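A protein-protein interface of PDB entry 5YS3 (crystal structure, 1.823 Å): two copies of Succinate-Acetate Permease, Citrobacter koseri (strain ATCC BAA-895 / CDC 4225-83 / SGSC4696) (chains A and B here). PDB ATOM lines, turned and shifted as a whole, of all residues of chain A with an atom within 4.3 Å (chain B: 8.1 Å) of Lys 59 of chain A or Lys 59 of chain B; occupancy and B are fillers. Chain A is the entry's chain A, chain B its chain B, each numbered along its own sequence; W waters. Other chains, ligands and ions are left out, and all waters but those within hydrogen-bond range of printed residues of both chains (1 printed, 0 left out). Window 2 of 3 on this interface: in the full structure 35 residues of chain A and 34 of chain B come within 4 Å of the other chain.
The backbone carbonyl oxygen of Leu 56 of chain A lies within hydrogen-bond range of the side-chain hydroxyl of Tyr 58 of chain B (2.6 Å).
The backbone carbonyl oxygen of Leu 6 of chain A sits at hydrogen-bond distance from the side-chain amino group of Lys 60 of chain A (2.9 Å).
Tyr 58 of chain B touches Leu 6 of chain A.
Lys 59 of chain B touches Leu 6 of chain A.
CD1 of Leu 66 of chain B touches CD1 of Leu 56 of chain A (3.8 Å).
Lys 59 of chain A touches Tyr 58 of chain B.
Lys 59 of chain A touches Lys 59 of chain B.
OH of Tyr 58 of chain B touches CG of Lys 60 of chain A, at 3.7 Å.
Printed residues of chain B within 4 Å of Lys 59 of chain A: Tyr 58 and Lys 59.
Of the printed residues of chain A, Tyr 58 of chain B touches Leu 6 (3.5 Å), Leu 56 (2.6 Å), Lys 59 (3.4 Å) and Lys 60 (3.7 Å).
Of chain A, only Leu 6 (3.9 Å) and Lys 59 (3.7 Å) come within 4 Å of Lys 59 of chain B.
Asn 62 of chain B touches none of the printed residues of chain A.
Printed residues of chain A within 4 Å of Leu 66 of chain B: Leu 56 (3.8 Å).
Hydrophobic or aromatic side chains of chain A within 4 Å of the printed part of chain B: Leu 6 and Leu 56.
Hydrophobic or aromatic side chains of chain B within 4 Å of the printed part of chain A: Tyr 58 and Leu 66.
Among the printed residues, no Asp or Glu carboxylate lies within 4 Å of a Lys or Arg side-chain nitrogen of the other chain.
Leu 6 of chain A touches Lys 59 of chain B, but with the chains exchanged Lys 59 of chain A does not touch Leu 6 of chain B (10.0 Å).
Leu 56 of chain A touches Tyr 58 of chain B, but with the chains exchanged Tyr 58 of chain A does not touch Leu 56 of chain B (14.5 Å).
Lys 59 of chain B touches its own counterpart, Lys 59 of chain A.
Lys 60 of chain A touches Tyr 58 of chain B, but with the chains exchanged Tyr 58 of chain A does not touch Lys 60 of chain B (14.3 Å).
Positions printed for both chains: 6, 56, 57, 58, 59, 60 and 61.
Of the 7 pairs that touch across the chains among the printed residues, 1 has its exchanged pair printed and touching as well.
Water W1 bridges N of Lys 59 of chain A (2.9 Å) and OH of Tyr 58 of chain B (3.5 Å).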
ATOM      1  N   LEU A   6      30.204  21.683 -26.576  1.00  0.00           N
ATOM      2  CA  LEU A   6      29.934  22.985 -27.163  1.00  0.00           C
ATOM      3  C   LEU A   6      28.807  22.914 -28.170  1.00  0.00           C
ATOM      4  O   LEU A   6      28.611  21.894 -28.816  1.00  0.00           O
ATOM      5  CB  LEU A   6      31.199  23.535 -27.826  1.00  0.00           C
ATOM      6  CG  LEU A   6      32.364  23.630 -26.830  1.00  0.00           C
ATOM      7  CD1 LEU A   6      33.676  23.953 -27.543  1.00  0.00           C
ATOM      8  CD2 LEU A   6      32.054  24.658 -25.777  1.00  0.00           C
ATOM      9  N   LEU A  56      33.627  29.910 -34.120  1.00  0.00           N
ATOM     10  CA  LEU A  56      33.138  28.964 -33.122  1.00  0.00           C
ATOM     11  C   LEU A  56      33.499  27.528 -33.508  1.00  0.00           C
ATOM     12  O   LEU A  56      33.408  26.602 -32.679  1.00  0.00           O
ATOM     13  CB  LEU A  56      31.622  29.112 -32.942  1.00  0.00           C
ATOM     14  CG  LEU A  56      31.191  30.429 -32.285  1.00  0.00           C
ATOM     15  CD1 LEU A  56      29.681  30.560 -32.190  1.00  0.00           C
ATOM     16  CD2 LEU A  56      31.817  30.537 -30.900  1.00  0.00           C
ATOM     17  N   GLU A  57      33.904  27.325 -34.764  1.00  0.00           N
ATOM     18  CA  GLU A  57      34.329  25.982 -35.174  1.00  0.00           C
ATOM     19  C   GLU A  57      35.725  25.606 -34.663  1.00  0.00           C
ATOM     20  O   GLU A  57      36.109  24.431 -34.672  1.00  0.00           O
ATOM     21  CB  GLU A  57      34.284  25.834 -36.700  1.00  0.00           C
ATOM     22  CG  GLU A  57      32.877  25.867 -37.294  1.00  0.00           C
ATOM     23  CD  GLU A  57      32.073  24.588 -37.050  1.00  0.00           C
ATOM     24  OE1 GLU A  57      32.443  23.772 -36.204  1.00  0.00           O
ATOM     25  OE2 GLU A  57      31.035  24.397 -37.710  1.00  0.00           O
ATOM     26  N   TYR A  58      36.479  26.596 -34.210  1.00  0.00           N
ATOM     27  CA  TYR A  58      37.865  26.381 -33.812  1.00  0.00           C
ATOM     28  C   TYR A  58      37.995  25.448 -32.619  1.00  0.00           C
ATOM     29  O   TYR A  58      38.781  24.474 -32.645  1.00  0.00           O
ATOM     30  CB  TYR A  58      38.506  27.731 -33.516  1.00  0.00           C
ATOM     31  CG  TYR A  58      39.902  27.760 -32.935  1.00  0.00           C
ATOM     32  CD1 TYR A  58      41.030  27.504 -33.724  1.00  0.00           C
ATOM     33  CD2 TYR A  58      40.101  28.149 -31.619  1.00  0.00           C
ATOM     34  CE1 TYR A  58      42.320  27.604 -33.183  1.00  0.00           C
ATOM     35  CE2 TYR A  58      41.369  28.248 -31.078  1.00  0.00           C
ATOM     36  CZ  TYR A  58      42.475  27.988 -31.856  1.00  0.00           C
ATOM     37  OH  TYR A  58      43.747  28.111 -31.276  1.00  0.00           O
ATOM     38  N   LYS A  59      37.213  25.725 -31.581  1.00  0.00           N
ATOM     39  CA  LYS A  59      37.277  24.899 -30.387  1.00  0.00           C
ATOM     40  C   LYS A  59      36.582  23.562 -30.595  1.00  0.00           C
ATOM     41  O   LYS A  59      36.758  22.645 -29.792  1.00  0.00           O
ATOM     42  CB  LYS A  59      36.671  25.626 -29.192  1.00  0.00           C
ATOM     43  CG  LYS A  59      37.592  26.683 -28.581  1.00  0.00           C
ATOM     44  CD  LYS A  59      36.969  27.291 -27.311  1.00  0.00           C
ATOM     45  CE  LYS A  59      37.848  28.393 -26.713  1.00  0.00           C
ATOM     46  NZ  LYS A  59      37.217  29.044 -25.525  1.00  0.00           N
ATOM     47  N   LYS A  60      35.800  23.443 -31.664  1.00  0.00           N
ATOM     48  CA  LYS A  60      35.202  22.155 -31.996  1.00  0.00           C
ATOM     49  C   LYS A  60      36.161  21.291 -32.816  1.00  0.00           C
ATOM     50  O   LYS A  60      35.843  20.156 -33.174  1.00  0.00           O
ATOM     51  CB  LYS A  60      33.898  22.339 -32.782  1.00  0.00           C
ATOM     52  CG  LYS A  60      32.946  23.389 -32.212  1.00  0.00           C
ATOM     53  CD  LYS A  60      31.879  22.794 -31.390  1.00  0.00           C
ATOM     54  CE  LYS A  60      30.941  21.946 -32.241  1.00  0.00           C
ATOM     55  NZ  LYS A  60      30.043  21.235 -31.301  1.00  0.00           N
ATOM     56  N   GLY A  61      37.322  21.836 -33.141  1.00  0.00           N
ATOM     57  CA  GLY A  61      38.299  21.082 -33.896  1.00  0.00           C
ATOM     58  C   GLY A  61      37.954  20.928 -35.361  1.00  0.00           C
ATOM     59  O   GLY A  61      38.465  20.032 -36.027  1.00  0.00           O
ATOM     60  N   LYS B   5      27.430  25.695 -14.522  1.00  0.00           N
ATOM     61  CA  LYS B   5      27.604  26.781 -13.562  1.00  0.00           C
ATOM     62  C   LYS B   5      27.575  28.135 -14.270  1.00  0.00           C
ATOM     63  O   LYS B   5      27.577  29.165 -13.620  1.00  0.00           O
ATOM     64  CB  LYS B   5      28.917  26.618 -12.792  1.00  0.00           C
ATOM     65  CG  LYS B   5      28.899  27.232 -11.403  1.00  0.00           C
ATOM     66  CD  LYS B   5      30.105  26.796 -10.580  1.00  0.00           C
ATOM     67  CE  LYS B   5      31.403  27.254 -11.229  1.00  0.00           C
ATOM     68  NZ  LYS B   5      32.290  27.907 -10.229  1.00  0.00           N
ATOM     69  N   LEU B   6      27.559  28.128 -15.602  1.00  0.00           N
ATOM     70  CA  LEU B   6      27.501  29.385 -16.363  1.00  0.00           C
ATOM     71  C   LEU B   6      26.133  30.012 -16.249  1.00  0.00           C
ATOM     72  O   LEU B   6      25.137  29.307 -16.094  1.00  0.00           O
ATOM     73  CB  LEU B   6      27.846  29.140 -17.828  1.00  0.00           C
ATOM     74  CG  LEU B   6      29.221  28.493 -18.032  1.00  0.00           C
ATOM     75  CD1 LEU B   6      29.349  27.995 -19.457  1.00  0.00           C
ATOM     76  CD2 LEU B   6      30.318  29.502 -17.720  1.00  0.00           C
ATOM     77  N   ALA B   7      26.077  31.336 -16.308  1.00  0.00           N
ATOM     78  CA  ALA B   7      24.808  32.049 -16.208  1.00  0.00           C
ATOM     79  C   ALA B   7      23.900  31.697 -17.370  1.00  0.00           C
ATOM     80  O   ALA B   7      24.368  31.273 -18.431  1.00  0.00           O
ATOM     81  CB  ALA B   7      25.038  33.545 -16.173  1.00  0.00           C
ATOM     82  N   PRO B   9      21.885  32.954 -20.363  1.00  0.00           N
ATOM     83  CA  PRO B   9      21.810  34.172 -21.170  1.00  0.00           C
ATOM     84  C   PRO B   9      20.472  34.336 -21.893  1.00  0.00           C
ATOM     85  O   PRO B   9      20.280  35.336 -22.587  1.00  0.00           O
ATOM     86  CB  PRO B   9      22.947  33.967 -22.179  1.00  0.00           C
ATOM     87  CG  PRO B   9      22.840  32.466 -22.468  1.00  0.00           C
ATOM     88  CD  PRO B   9      22.504  31.839 -21.111  1.00  0.00           C
ATOM     89  N   GLY B  54      23.182  35.063 -27.772  1.00  0.00           N
ATOM     90  CA  GLY B  54      23.381  33.909 -28.655  1.00  0.00           C
ATOM     91  C   GLY B  54      24.759  33.282 -28.492  1.00  0.00           C
ATOM     92  O   GLY B  54      24.901  32.078 -28.329  1.00  0.00           O
ATOM     93  N   LEU B  55      25.790  34.117 -28.525  1.00  0.00           N
ATOM     94  CA  LEU B  55      27.154  33.617 -28.406  1.00  0.00           C
ATOM     95  C   LEU B  55      27.384  32.966 -27.041  1.00  0.00           C
ATOM     96  O   LEU B  55      28.185  32.043 -26.910  1.00  0.00           O
ATOM     97  CB  LEU B  55      28.159  34.761 -28.629  1.00  0.00           C
ATOM     98  CG  LEU B  55      28.053  35.375 -30.029  1.00  0.00           C
ATOM     99  CD1 LEU B  55      28.925  36.666 -30.178  1.00  0.00           C
ATOM    100  CD2 LEU B  55      28.393  34.340 -31.103  1.00  0.00           C
ATOM    101  N   LEU B  56      26.697  33.466 -26.014  1.00  0.00           N
ATOM    102  CA  LEU B  56      26.853  32.895 -24.679  1.00  0.00           C
ATOM    103  C   LEU B  56      26.199  31.501 -24.550  1.00  0.00           C
ATOM    104  O   LEU B  56      26.466  30.767 -23.585  1.00  0.00           O
ATOM    105  CB  LEU B  56      26.279  33.865 -23.626  1.00  0.00           C
ATOM    106  CG  LEU B  56      27.072  35.165 -23.437  1.00  0.00           C
ATOM    107  CD1 LEU B  56      26.365  36.127 -22.421  1.00  0.00           C
ATOM    108  CD2 LEU B  56      28.504  34.844 -23.003  1.00  0.00           C
ATOM    109  N   GLU B  57      25.377  31.119 -25.529  1.00  0.00           N
ATOM    110  CA  GLU B  57      24.768  29.772 -25.513  1.00  0.00           C
ATOM    111  C   GLU B  57      25.735  28.699 -25.978  1.00  0.00           C
ATOM    112  O   GLU B  57      25.487  27.507 -25.788  1.00  0.00           O
ATOM    113  CB  GLU B  57      23.516  29.720 -26.401  1.00  0.00           C
ATOM    114  CG  GLU B  57      22.404  30.594 -25.910  1.00  0.00           C
ATOM    115  CD  GLU B  57      21.655  29.976 -24.746  1.00  0.00           C
ATOM    116  OE1 GLU B  57      22.195  29.074 -24.070  1.00  0.00           O
ATOM    117  OE2 GLU B  57      20.536  30.442 -24.475  1.00  0.00           O
ATOM    118  N   TYR B  58      26.834  29.130 -26.596  1.00  0.00           N
ATOM    119  CA  TYR B  58      27.813  28.213 -27.187  1.00  0.00           C
ATOM    120  C   TYR B  58      28.439  27.316 -26.135  1.00  0.00           C
ATOM    121  O   TYR B  58      28.448  26.102 -26.269  1.00  0.00           O
ATOM    122  CB  TYR B  58      28.889  29.012 -27.902  1.00  0.00           C
ATOM    123  CG  TYR B  58      30.077  28.246 -28.450  1.00  0.00           C
ATOM    124  CD1 TYR B  58      29.948  27.406 -29.567  1.00  0.00           C
ATOM    125  CD2 TYR B  58      31.349  28.425 -27.908  1.00  0.00           C
ATOM    126  CE1 TYR B  58      31.052  26.747 -30.098  1.00  0.00           C
ATOM    127  CE2 TYR B  58      32.457  27.777 -28.432  1.00  0.00           C
ATOM    128  CZ  TYR B  58      32.306  26.947 -29.523  1.00  0.00           C
ATOM    129  OH  TYR B  58      33.403  26.310 -30.049  1.00  0.00           O
ATOM    130  N   LYS B  59      28.959  27.913 -25.071  1.00  0.00           N
ATOM    131  CA  LYS B  59      29.582  27.101 -24.047  1.00  0.00           C
ATOM    132  C   LYS B  59      28.549  26.383 -23.183  1.00  0.00           C
ATOM    133  O   LYS B  59      28.887  25.468 -22.451  1.00  0.00           O
ATOM    134  CB  LYS B  59      30.504  27.951 -23.171  1.00  0.00           C
ATOM    135  CG  LYS B  59      31.788  28.350 -23.872  1.00  0.00           C
ATOM    136  CD  LYS B  59      32.728  29.085 -22.914  1.00  0.00           C
ATOM    137  CE  LYS B  59      34.053  29.409 -23.589  1.00  0.00           C
ATOM    138  NZ  LYS B  59      35.032  30.022 -22.636  1.00  0.00           N
ATOM    139  N   LYS B  60      27.294  26.802 -23.261  1.00  0.00           N
ATOM    140  CA  LYS B  60      26.233  26.091 -22.564  1.00  0.00           C
ATOM    141  C   LYS B  60      25.737  24.894 -23.372  1.00  0.00           C
ATOM    142  O   LYS B  60      24.841  24.174 -22.938  1.00  0.00           O
ATOM    143  CB  LYS B  60      25.078  27.045 -22.238  1.00  0.00           C
ATOM    144  CG  LYS B  60      25.510  28.092 -21.186  1.00  0.00           C
ATOM    145  CD  LYS B  60      24.363  28.857 -20.610  1.00  0.00           C
ATOM    146  CE  LYS B  60      23.515  28.004 -19.684  1.00  0.00           C
ATOM    147  NZ  LYS B  60      24.033  27.976 -18.297  1.00  0.00           N
ATOM    148  N   GLY B  61      26.324  24.676 -24.545  1.00  0.00           N
ATOM    149  CA  GLY B  61      25.970  23.519 -25.345  1.00  0.00           C
ATOM    150  C   GLY B  61      24.598  23.627 -25.972  1.00  0.00           C
ATOM    151  O   GLY B  61      24.002  22.614 -26.327  1.00  0.00           O
ATOM    152  N   ASN B  62      24.088  24.849 -26.118  1.00  0.00           N
ATOM    153  CA  ASN B  62      22.700  25.023 -26.551  1.00  0.00           C
ATOM    154  C   ASN B  62      22.636  25.508 -27.996  1.00  0.00           C
ATOM    155  O   ASN B  62      22.612  26.702 -28.277  1.00  0.00           O
ATOM    156  CB  ASN B  62      21.959  25.993 -25.611  1.00  0.00           C
ATOM    157  CG  ASN B  62      20.474  26.167 -25.974  1.00  0.00           C
ATOM    158  OD1 ASN B  62      20.019  25.722 -27.016  1.00  0.00           O
ATOM    159  ND2 ASN B  62      19.728  26.834 -25.102  1.00  0.00           N
ATOM    160  N   LEU B  66      21.942  29.319 -29.505  1.00  0.00           N
ATOM    161  CA  LEU B  66      22.983  29.954 -30.306  1.00  0.00           C
ATOM    162  C   LEU B  66      22.414  30.356 -31.665  1.00  0.00           C
ATOM    163  O   LEU B  66      22.656  31.455 -32.164  1.00  0.00           O
ATOM    164  CB  LEU B  66      24.175  29.005 -30.499  1.00  0.00           C
ATOM    165  CG  LEU B  66      25.278  29.365 -31.512  1.00  0.00           C
ATOM    166  CD1 LEU B  66      26.055  30.649 -31.176  1.00  0.00           C
ATOM    167  CD2 LEU B  66      26.259  28.174 -31.638  1.00  0.00           C
HETATM  168  O   HOH W   1      36.043  28.345 -31.084  1.00  0.00           O
